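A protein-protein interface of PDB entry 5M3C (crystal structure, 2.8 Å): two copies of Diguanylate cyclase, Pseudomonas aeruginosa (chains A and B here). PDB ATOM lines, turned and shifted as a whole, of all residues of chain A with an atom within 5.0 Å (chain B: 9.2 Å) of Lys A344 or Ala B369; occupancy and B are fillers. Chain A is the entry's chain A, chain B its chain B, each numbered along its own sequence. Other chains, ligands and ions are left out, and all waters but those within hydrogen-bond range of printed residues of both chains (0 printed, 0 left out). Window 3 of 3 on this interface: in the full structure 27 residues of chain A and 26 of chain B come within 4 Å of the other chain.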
ATOM      1  N   LEU A 340     -29.421  26.458  -9.499  1.00  0.00           N
ATOM      2  CA  LEU A 340     -28.016  26.073  -9.511  1.00  0.00           C
ATOM      3  C   LEU A 340     -27.382  26.382 -10.863  1.00  0.00           C
ATOM      4  O   LEU A 340     -26.272  26.914 -10.931  1.00  0.00           O
ATOM      5  CB  LEU A 340     -27.862  24.587  -9.189  1.00  0.00           C
ATOM      6  CG  LEU A 340     -28.488  24.128  -7.870  1.00  0.00           C
ATOM      7  CD1 LEU A 340     -28.014  22.727  -7.518  1.00  0.00           C
ATOM      8  CD2 LEU A 340     -28.163  25.099  -6.745  1.00  0.00           C
ATOM      9  N   SER A 341     -28.094  26.050 -11.936  1.00  0.00           N
ATOM     10  CA  SER A 341     -27.615  26.325 -13.287  1.00  0.00           C
ATOM     11  C   SER A 341     -27.295  27.805 -13.453  1.00  0.00           C
ATOM     12  O   SER A 341     -26.234  28.170 -13.954  1.00  0.00           O
ATOM     13  CB  SER A 341     -28.663  25.913 -14.321  1.00  0.00           C
ATOM     14  OG  SER A 341     -28.215  26.202 -15.635  1.00  0.00           O
ATOM     15  N   TYR A 342     -28.223  28.652 -13.023  1.00  0.00           N
ATOM     16  CA  TYR A 342     -28.068  30.094 -13.164  1.00  0.00           C
ATOM     17  C   TYR A 342     -27.022  30.634 -12.198  1.00  0.00           C
ATOM     18  O   TYR A 342     -26.358  31.627 -12.487  1.00  0.00           O
ATOM     19  CB  TYR A 342     -29.408  30.791 -12.929  1.00  0.00           C
ATOM     20  CG  TYR A 342     -29.374  32.284 -13.161  1.00  0.00           C
ATOM     21  CD1 TYR A 342     -28.887  32.810 -14.350  1.00  0.00           C
ATOM     22  CD2 TYR A 342     -29.843  33.168 -12.197  1.00  0.00           C
ATOM     23  CE1 TYR A 342     -28.857  34.173 -14.568  1.00  0.00           C
ATOM     24  CE2 TYR A 342     -29.819  34.533 -12.407  1.00  0.00           C
ATOM     25  CZ  TYR A 342     -29.327  35.030 -13.595  1.00  0.00           C
ATOM     26  OH  TYR A 342     -29.301  36.389 -13.808  1.00  0.00           O
ATOM     27  N   LEU A 343     -26.876  29.976 -11.054  1.00  0.00           N
ATOM     28  CA  LEU A 343     -25.928  30.416 -10.040  1.00  0.00           C
ATOM     29  C   LEU A 343     -24.500  30.367 -10.570  1.00  0.00           C
ATOM     30  O   LEU A 343     -23.683  31.225 -10.245  1.00  0.00           O
ATOM     31  CB  LEU A 343     -26.046  29.553  -8.783  1.00  0.00           C
ATOM     32  CG  LEU A 343     -25.291  30.063  -7.554  1.00  0.00           C
ATOM     33  CD1 LEU A 343     -25.887  31.367  -7.045  1.00  0.00           C
ATOM     34  CD2 LEU A 343     -25.292  29.013  -6.455  1.00  0.00           C
ATOM     35  N   LYS A 344     -24.204  29.366 -11.390  1.00  0.00           N
ATOM     36  CA  LYS A 344     -22.860  29.210 -11.930  1.00  0.00           C
ATOM     37  C   LYS A 344     -22.611  30.216 -13.054  1.00  0.00           C
ATOM     38  O   LYS A 344     -21.529  30.793 -13.146  1.00  0.00           O
ATOM     39  CB  LYS A 344     -22.644  27.782 -12.441  1.00  0.00           C
ATOM     40  CG  LYS A 344     -21.229  27.249 -12.238  1.00  0.00           C
ATOM     41  CD  LYS A 344     -20.174  28.338 -12.387  1.00  0.00           C
ATOM     42  CE  LYS A 344     -18.770  27.766 -12.481  1.00  0.00           C
ATOM     43  NZ  LYS A 344     -18.464  26.831 -11.364  1.00  0.00           N
ATOM     44  N   ARG A 345     -23.617  30.428 -13.900  1.00  0.00           N
ATOM     45  CA  ARG A 345     -23.498  31.360 -15.025  1.00  0.00           C
ATOM     46  C   ARG A 345     -23.224  32.794 -14.571  1.00  0.00           C
ATOM     47  O   ARG A 345     -22.734  33.609 -15.351  1.00  0.00           O
ATOM     48  CB  ARG A 345     -24.755  31.315 -15.908  1.00  0.00           C
ATOM     49  CG  ARG A 345     -24.691  30.269 -17.015  1.00  0.00           C
ATOM     50  CD  ARG A 345     -25.894  30.317 -17.952  1.00  0.00           C
ATOM     51  NE  ARG A 345     -26.915  29.328 -17.602  1.00  0.00           N
ATOM     52  CZ  ARG A 345     -28.157  29.618 -17.218  1.00  0.00           C
ATOM     53  NH1 ARG A 345     -28.564  30.879 -17.137  1.00  0.00           N
ATOM     54  NH2 ARG A 345     -29.003  28.636 -16.921  1.00  0.00           N
ATOM     55  N   LEU A 346     -23.538  33.094 -13.313  1.00  0.00           N
ATOM     56  CA  LEU A 346     -23.289  34.419 -12.748  1.00  0.00           C
ATOM     57  C   LEU A 346     -21.813  34.600 -12.408  1.00  0.00           C
ATOM     58  O   LEU A 346     -21.209  33.724 -11.786  1.00  0.00           O
ATOM     59  CB  LEU A 346     -24.124  34.632 -11.482  1.00  0.00           C
ATOM     60  CG  LEU A 346     -25.647  34.618 -11.637  1.00  0.00           C
ATOM     61  CD1 LEU A 346     -26.325  34.609 -10.276  1.00  0.00           C
ATOM     62  CD2 LEU A 346     -26.119  35.804 -12.460  1.00  0.00           C
ATOM     63  N   PRO A 347     -21.230  35.743 -12.812  1.00  0.00           N
ATOM     64  CA  PRO A 347     -19.842  36.052 -12.501  1.00  0.00           C
ATOM     65  C   PRO A 347     -19.715  36.577 -11.082  1.00  0.00           C
ATOM     66  O   PRO A 347     -19.602  37.785 -10.873  1.00  0.00           O
ATOM     67  CB  PRO A 347     -19.504  37.148 -13.504  1.00  0.00           C
ATOM     68  CG  PRO A 347     -20.791  37.867 -13.704  1.00  0.00           C
ATOM     69  CD  PRO A 347     -21.876  36.834 -13.567  1.00  0.00           C
ATOM     70  N   SER A 380     -17.444  24.484  -4.408  1.00  0.00           N
ATOM     71  CA  SER A 380     -17.584  23.783  -5.674  1.00  0.00           C
ATOM     72  C   SER A 380     -17.686  24.751  -6.848  1.00  0.00           C
ATOM     73  O   SER A 380     -17.183  24.466  -7.935  1.00  0.00           O
ATOM     74  CB  SER A 380     -18.821  22.890  -5.647  1.00  0.00           C
ATOM     75  OG  SER A 380     -19.082  22.361  -6.933  1.00  0.00           O
ATOM     76  N   MET A 381     -18.342  25.888  -6.627  1.00  0.00           N
ATOM     77  CA  MET A 381     -18.518  26.881  -7.683  1.00  0.00           C
ATOM     78  C   MET A 381     -17.461  27.983  -7.591  1.00  0.00           C
ATOM     79  O   MET A 381     -17.647  29.078  -8.125  1.00  0.00           O
ATOM     80  CB  MET A 381     -19.924  27.491  -7.631  1.00  0.00           C
ATOM     81  CG  MET A 381     -21.030  26.500  -7.285  1.00  0.00           C
ATOM     82  SD  MET A 381     -22.552  26.681  -8.246  1.00  0.00           S
ATOM     83  CE  MET A 381     -22.608  28.449  -8.510  1.00  0.00           C
ATOM     84  N   GLN A 382     -16.352  27.677  -6.918  1.00  0.00           N
ATOM     85  CA  GLN A 382     -15.237  28.612  -6.754  1.00  0.00           C
ATOM     86  C   GLN A 382     -15.688  29.999  -6.289  1.00  0.00           C
ATOM     87  O   GLN A 382     -15.336  31.011  -6.893  1.00  0.00           O
ATOM     88  CB  GLN A 382     -14.434  28.726  -8.056  1.00  0.00           C
ATOM     89  CG  GLN A 382     -13.744  27.437  -8.478  1.00  0.00           C
ATOM     90  CD  GLN A 382     -14.711  26.400  -9.017  1.00  0.00           C
ATOM     91  OE1 GLN A 382     -15.519  26.687  -9.905  1.00  0.00           O
ATOM     92  NE2 GLN A 382     -14.631  25.181  -8.489  1.00  0.00           N
ATOM     93  N   ILE B 353     -29.257  12.911 -10.478  1.00  0.00           N
ATOM     94  CA  ILE B 353     -28.809  14.020 -11.315  1.00  0.00           C
ATOM     95  C   ILE B 353     -29.472  13.952 -12.686  1.00  0.00           C
ATOM     96  O   ILE B 353     -29.378  12.937 -13.372  1.00  0.00           O
ATOM     97  CB  ILE B 353     -27.281  14.005 -11.512  1.00  0.00           C
ATOM     98  CG1 ILE B 353     -26.568  13.880 -10.162  1.00  0.00           C
ATOM     99  CG2 ILE B 353     -26.832  15.261 -12.248  1.00  0.00           C
ATOM    100  CD1 ILE B 353     -25.058  13.840 -10.263  1.00  0.00           C
ATOM    101  N   PHE B 357     -27.412  17.345 -17.549  1.00  0.00           N
ATOM    102  CA  PHE B 357     -26.074  17.717 -17.093  1.00  0.00           C
ATOM    103  C   PHE B 357     -25.049  16.623 -17.356  1.00  0.00           C
ATOM    104  O   PHE B 357     -23.863  16.899 -17.512  1.00  0.00           O
ATOM    105  CB  PHE B 357     -26.087  18.035 -15.598  1.00  0.00           C
ATOM    106  CG  PHE B 357     -27.100  19.071 -15.211  1.00  0.00           C
ATOM    107  CD1 PHE B 357     -27.021  20.358 -15.720  1.00  0.00           C
ATOM    108  CD2 PHE B 357     -28.127  18.763 -14.335  1.00  0.00           C
ATOM    109  CE1 PHE B 357     -27.950  21.316 -15.368  1.00  0.00           C
ATOM    110  CE2 PHE B 357     -29.060  19.715 -13.977  1.00  0.00           C
ATOM    111  CZ  PHE B 357     -28.972  20.995 -14.495  1.00  0.00           C
ATOM    112  N   GLY B 360     -23.666  15.976 -21.319  1.00  0.00           N
ATOM    113  CA  GLY B 360     -22.669  16.889 -21.871  1.00  0.00           C
ATOM    114  C   GLY B 360     -21.256  16.558 -21.428  1.00  0.00           C
ATOM    115  O   GLY B 360     -20.282  17.077 -21.978  1.00  0.00           O
ATOM    116  N   LEU B 361     -21.143  15.685 -20.431  1.00  0.00           N
ATOM    117  CA  LEU B 361     -19.846  15.326 -19.868  1.00  0.00           C
ATOM    118  C   LEU B 361     -18.967  14.619 -20.900  1.00  0.00           C
ATOM    119  O   LEU B 361     -19.447  13.769 -21.651  1.00  0.00           O
ATOM    120  CB  LEU B 361     -20.031  14.429 -18.642  1.00  0.00           C
ATOM    121  CG  LEU B 361     -20.864  15.012 -17.497  1.00  0.00           C
ATOM    122  CD1 LEU B 361     -21.080  13.968 -16.412  1.00  0.00           C
ATOM    123  CD2 LEU B 361     -20.207  16.253 -16.917  1.00  0.00           C
ATOM    124  N   PRO B 362     -17.684  14.971 -20.943  1.00  0.00           N
ATOM    125  CA  PRO B 362     -17.120  15.993 -20.068  1.00  0.00           C
ATOM    126  C   PRO B 362     -16.693  17.241 -20.839  1.00  0.00           C
ATOM    127  O   PRO B 362     -16.052  18.126 -20.274  1.00  0.00           O
ATOM    128  CB  PRO B 362     -15.899  15.292 -19.478  1.00  0.00           C
ATOM    129  CG  PRO B 362     -15.451  14.361 -20.555  1.00  0.00           C
ATOM    130  CD  PRO B 362     -16.670  13.985 -21.358  1.00  0.00           C
ATOM    131  N   ASP B 363     -17.058  17.305 -22.117  1.00  0.00           N
ATOM    132  CA  ASP B 363     -16.628  18.395 -22.987  1.00  0.00           C
ATOM    133  C   ASP B 363     -17.212  19.736 -22.545  1.00  0.00           C
ATOM    134  O   ASP B 363     -16.503  20.742 -22.494  1.00  0.00           O
ATOM    135  CB  ASP B 363     -17.021  18.103 -24.439  1.00  0.00           C
ATOM    136  N   ASP B 364     -18.504  19.746 -22.224  1.00  0.00           N
ATOM    137  CA  ASP B 364     -19.184  20.980 -21.832  1.00  0.00           C
ATOM    138  C   ASP B 364     -18.730  21.430 -20.444  1.00  0.00           C
ATOM    139  O   ASP B 364     -18.807  20.663 -19.485  1.00  0.00           O
ATOM    140  CB  ASP B 364     -20.703  20.791 -21.859  1.00  0.00           C
ATOM    141  CG  ASP B 364     -21.461  22.108 -21.787  1.00  0.00           C
ATOM    142  OD1 ASP B 364     -21.301  22.843 -20.790  1.00  0.00           O
ATOM    143  OD2 ASP B 364     -22.228  22.404 -22.727  1.00  0.00           O
ATOM    144  N   PRO B 365     -18.256  22.682 -20.337  1.00  0.00           N
ATOM    145  CA  PRO B 365     -17.735  23.204 -19.071  1.00  0.00           C
ATOM    146  C   PRO B 365     -18.832  23.440 -18.034  1.00  0.00           C
ATOM    147  O   PRO B 365     -18.642  23.145 -16.854  1.00  0.00           O
ATOM    148  CB  PRO B 365     -17.080  24.540 -19.465  1.00  0.00           C
ATOM    149  CG  PRO B 365     -17.257  24.695 -20.943  1.00  0.00           C
ATOM    150  CD  PRO B 365     -18.287  23.708 -21.392  1.00  0.00           C
ATOM    151  N   HIS B 366     -19.965  23.970 -18.485  1.00  0.00           N
ATOM    152  CA  HIS B 366     -21.086  24.285 -17.605  1.00  0.00           C
ATOM    153  C   HIS B 366     -21.673  23.031 -16.966  1.00  0.00           C
ATOM    154  O   HIS B 366     -21.855  22.973 -15.752  1.00  0.00           O
ATOM    155  CB  HIS B 366     -22.175  25.020 -18.389  1.00  0.00           C
ATOM    156  CG  HIS B 366     -23.433  25.244 -17.611  1.00  0.00           C
ATOM    157  ND1 HIS B 366     -23.615  26.337 -16.791  1.00  0.00           N
ATOM    158  CD2 HIS B 366     -24.574  24.519 -17.531  1.00  0.00           C
ATOM    159  CE1 HIS B 366     -24.815  26.274 -16.238  1.00  0.00           C
ATOM    160  NE2 HIS B 366     -25.417  25.180 -16.670  1.00  0.00           N
ATOM    161  N   ASP B 367     -21.973  22.035 -17.792  1.00  0.00           N
ATOM    162  CA  ASP B 367     -22.561  20.789 -17.306  1.00  0.00           C
ATOM    163  C   ASP B 367     -21.638  20.090 -16.313  1.00  0.00           C
ATOM    164  O   ASP B 367     -22.101  19.384 -15.417  1.00  0.00           O
ATOM    165  CB  ASP B 367     -22.881  19.853 -18.474  1.00  0.00           C
ATOM    166  CG  ASP B 367     -24.143  20.255 -19.220  1.00  0.00           C
ATOM    167  OD1 ASP B 367     -24.809  21.227 -18.801  1.00  0.00           O
ATOM    168  OD2 ASP B 367     -24.473  19.592 -20.227  1.00  0.00           O
ATOM    169  N   ALA B 368     -20.334  20.287 -16.477  1.00  0.00           N
ATOM    170  CA  ALA B 368     -19.358  19.723 -15.552  1.00  0.00           C
ATOM    171  C   ALA B 368     -19.469  20.404 -14.194  1.00  0.00           C
ATOM    172  O   ALA B 368     -19.532  19.740 -13.159  1.00  0.00           O
ATOM    173  CB  ALA B 368     -17.950  19.877 -16.109  1.00  0.00           C
ATOM    174  N   ALA B 369     -19.500  21.734 -14.210  1.00  0.00           N
ATOM    175  CA  ALA B 369     -19.573  22.530 -12.985  1.00  0.00           C
ATOM    176  C   ALA B 369     -20.798  22.161 -12.157  1.00  0.00           C
ATOM    177  O   ALA B 369     -20.708  21.967 -10.943  1.00  0.00           O
ATOM    178  CB  ALA B 369     -19.601  24.012 -13.327  1.00  0.00           C
ATOM    179  N   ILE B 370     -21.941  22.068 -12.827  1.00  0.00           N
ATOM    180  CA  ILE B 370     -23.196  21.730 -12.169  1.00  0.00           C
ATOM    181  C   ILE B 370     -23.174  20.313 -11.613  1.00  0.00           C
ATOM    182  O   ILE B 370     -23.595  20.086 -10.486  1.00  0.00           O
ATOM    183  CB  ILE B 370     -24.386  21.853 -13.135  1.00  0.00           C
ATOM    184  CG1 ILE B 370     -24.461  23.269 -13.709  1.00  0.00           C
ATOM    185  CG2 ILE B 370     -25.682  21.492 -12.427  1.00  0.00           C
ATOM    186  CD1 ILE B 370     -24.376  24.360 -12.664  1.00  0.00           C
ATOM    187  N   THR B 371     -22.697  19.361 -12.406  1.00  0.00           N
ATOM    188  CA  THR B 371     -22.618  17.977 -11.956  1.00  0.00           C
ATOM    189  C   THR B 371     -21.682  17.881 -10.757  1.00  0.00           C
ATOM    190  O   THR B 371     -21.951  17.159  -9.798  1.00  0.00           O
ATOM    191  CB  THR B 371     -22.123  17.040 -13.076  1.00  0.00           C
ATOM    192  OG1 THR B 371     -22.997  17.138 -14.208  1.00  0.00           O
ATOM    193  CG2 THR B 371     -22.084  15.599 -12.592  1.00  0.00           C
ATOM    194  N   ARG B 372     -20.584  18.625 -10.817  1.00  0.00           N
ATOM    195  CA  ARG B 372     -19.606  18.646  -9.737  1.00  0.00           C
ATOM    196  C   ARG B 372     -20.224  19.300  -8.498  1.00  0.00           C
ATOM    197  O   ARG B 372     -19.946  18.906  -7.367  1.00  0.00           O
ATOM    198  CB  ARG B 372     -18.357  19.406 -10.191  1.00  0.00           C
ATOM    199  CG  ARG B 372     -17.036  18.862  -9.668  1.00  0.00           C
ATOM    200  CD  ARG B 372     -15.934  19.057 -10.702  1.00  0.00           C
ATOM    201  NE  ARG B 372     -16.098  20.303 -11.452  1.00  0.00           N
ATOM    202  CZ  ARG B 372     -15.608  20.522 -12.670  1.00  0.00           C
ATOM    203  NH1 ARG B 372     -14.914  19.581 -13.300  1.00  0.00           N
ATOM    204  NH2 ARG B 372     -15.819  21.689 -13.266  1.00  0.00           N
ATOM    205  N   ALA B 373     -21.076  20.296  -8.726  1.00  0.00           N
ATOM    206  CA  ALA B 373     -21.772  20.980  -7.641  1.00  0.00           C
ATOM    207  C   ALA B 373     -22.799  20.074  -6.970  1.00  0.00           C
ATOM    208  O   ALA B 373     -22.846  19.974  -5.746  1.00  0.00           O
ATOM    209  CB  ALA B 373     -22.449  22.234  -8.168  1.00  0.00           C
ATOM    210  N   ILE B 374     -23.620  19.420  -7.781  1.00  0.00           N
ATOM    211  CA  ILE B 374     -24.669  18.540  -7.280  1.00  0.00           C
ATOM    212  C   ILE B 374     -24.100  17.411  -6.426  1.00  0.00           C
ATOM    213  O   ILE B 374     -24.682  17.051  -5.405  1.00  0.00           O
ATOM    214  CB  ILE B 374     -25.476  17.922  -8.434  1.00  0.00           C
ATOM    215  CG1 ILE B 374     -26.226  19.011  -9.200  1.00  0.00           C
ATOM    216  CG2 ILE B 374     -26.462  16.894  -7.904  1.00  0.00           C
ATOM    217  CD1 ILE B 374     -26.931  18.506 -10.439  1.00  0.00           C
ATOM    218  N   ILE B 375     -22.975  16.846  -6.851  1.00  0.00           N
ATOM    219  CA  ILE B 375     -22.330  15.777  -6.093  1.00  0.00           C
ATOM    220  C   ILE B 375     -21.914  16.301  -4.724  1.00  0.00           C
ATOM    221  O   ILE B 375     -22.231  15.699  -3.694  1.00  0.00           O
ATOM    222  CB  ILE B 375     -21.100  15.212  -6.835  1.00  0.00           C
ATOM    223  CG1 ILE B 375     -21.542  14.473  -8.103  1.00  0.00           C
ATOM    224  CG2 ILE B 375     -20.314  14.274  -5.926  1.00  0.00           C
ATOM    225  CD1 ILE B 375     -20.418  14.188  -9.076  1.00  0.00           C
ATOM    226  N   ALA B 376     -21.214  17.432  -4.722  1.00  0.00           N
ATOM    227  CA  ALA B 376     -20.779  18.070  -3.483  1.00  0.00           C
ATOM    228  C   ALA B 376     -21.980  18.384  -2.593  1.00  0.00           C
ATOM    229  O   ALA B 376     -21.912  18.261  -1.368  1.00  0.00           O
ATOM    230  CB  ALA B 376     -19.999  19.342  -3.789  1.00  0.00           C
ATOM    231  N   LEU B 377     -23.079  18.786  -3.223  1.00  0.00           N
ATOM    232  CA  LEU B 377     -24.309  19.112  -2.509  1.00  0.00           C
ATOM    233  C   LEU B 377     -24.898  17.866  -1.857  1.00  0.00           C
ATOM    234  O   LEU B 377     -25.167  17.850  -0.659  1.00  0.00           O
ATOM    235  CB  LEU B 377     -25.329  19.727  -3.469  1.00  0.00           C
ATOM    236  CG  LEU B 377     -26.364  20.667  -2.847  1.00  0.00           C
ATOM    237  CD1 LEU B 377     -27.312  21.190  -3.914  1.00  0.00           C
ATOM    238  CD2 LEU B 377     -27.142  19.982  -1.735  1.00  0.00           C
ATOM    239  N   PHE B 398     -15.430  10.584 -16.252  1.00  0.00           N
ATOM    240  CA  PHE B 398     -15.580  11.854 -15.544  1.00  0.00           C
ATOM    241  C   PHE B 398     -16.224  11.647 -14.178  1.00  0.00           C
ATOM    242  O   PHE B 398     -15.656  12.006 -13.147  1.00  0.00           O
ATOM    243  CB  PHE B 398     -16.438  12.814 -16.372  1.00  0.00           C
ATOM    244  CG  PHE B 398     -16.674  14.148 -15.716  1.00  0.00           C
ATOM    245  CD1 PHE B 398     -17.566  14.272 -14.661  1.00  0.00           C
ATOM    246  CD2 PHE B 398     -16.015  15.283 -16.165  1.00  0.00           C
ATOM    247  CE1 PHE B 398     -17.788  15.499 -14.065  1.00  0.00           C
ATOM    248  CE2 PHE B 398     -16.233  16.511 -15.572  1.00  0.00           C
ATOM    249  CZ  PHE B 398     -17.121  16.620 -14.520  1.00  0.00           C
ATOM    250  N   GLU B 402     -14.706  12.518 -10.311  1.00  0.00           N
ATOM    251  CA  GLU B 402     -15.383  13.599  -9.595  1.00  0.00           C
ATOM    252  C   GLU B 402     -16.181  13.090  -8.395  1.00  0.00           C
ATOM    253  O   GLU B 402     -16.939  13.841  -7.781  1.00  0.00           O
ATOM    254  CB  GLU B 402     -16.299  14.372 -10.544  1.00  0.00           C
ATOM    255  CG  GLU B 402     -15.570  15.026 -11.707  1.00  0.00           C
ATOM    256  CD  GLU B 402     -14.557  16.063 -11.259  1.00  0.00           C
ATOM    257  OE1 GLU B 402     -13.710  16.464 -12.085  1.00  0.00           O
ATOM    258  OE2 GLU B 402     -14.611  16.482 -10.083  1.00  0.00           O
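The side-chain hydroxyl (OG) of Ser A380 lies close to the backbone NH (N) of Ala B373 (3.4 Å).
The side-chain hydroxyl of Ser A341 is in hydrogen-bond range of a ring nitrogen (NE2) of His B366.
O of Ser A380 lies within hydrogen-bond range of NE2 of Gln A382, 2.7 Å away.
The side-chain carboxylate (OE1) of Glu B402 lies within salt-bridge range of the guanidinium group (NH1) of Arg B372.
The guanidinium group (NH2) of Arg A345 lies within hydrogen-bond range of the side-chain hydroxyl (OG) of Ser A341.
The side-chain amino group (NZ) of Lys A344 lies within hydrogen-bond range of the side-chain amide oxygen (OE1) of Gln A382, at 3.3 Å.
The side-chain carboxylate of Asp B364 is in hydrogen-bond range of the backbone NH of His B366 (2.9 Å).
Among the printed residues, pairs that only touch across the chains: Leu A340 with Ile B370 (3.6 Å), Leu A340 with Leu B377 (3.98 Å), Ser A341 with Ile B370 (3.8 Å), Lys A344 with Ala B369 (3.6 Å), Lys A344 with Ile B370 (3.8 Å), Arg A345 with His B366 (3.9 Å) and Ser A380 with Arg B372 (3.6 Å).
No residue of chain B comes within 4 Å of Leu A343.
No residue of chain B comes within 4 Å of Met A381.
Of the printed residues of chain A, Ile B370 touches Leu A340 (3.6 Å), Ser A341 (3.8 Å) and Lys A344 (3.8 Å).
Printed residues of chain B within 4 Å of Ser A341: His B366 (3.2 Å) and Ile B370 (3.8 Å).
Of the printed residues of chain A, Ala B373 touches Ser A380 (3.1 Å).
Of the printed residues of chain A, Arg B372 touches Ser A380.
Gln A382 touches none of the printed residues of chain B.
The nearest residue of chain B that does not touch Lys A344 is His B366 (4.6 Å).
The nearest residue of chain A that does not touch Ala B369 is Ser A380 (4.3 Å).
The nearest printed residue of chain B that does not touch Ser A341 is Phe B357 (4.8 Å).
Hydrophobic or aromatic side chains of chain A within 4 Å of the printed part of chain B: Leu A340.
Hydrophobic or aromatic side chains of chain B within 4 Å of the printed part of chain A: His B366, Ala B369, Ile B370, Ala B373 and Leu B377.
Among the printed residues, 9 pairs touch across the chains.
No position is printed for both chains.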
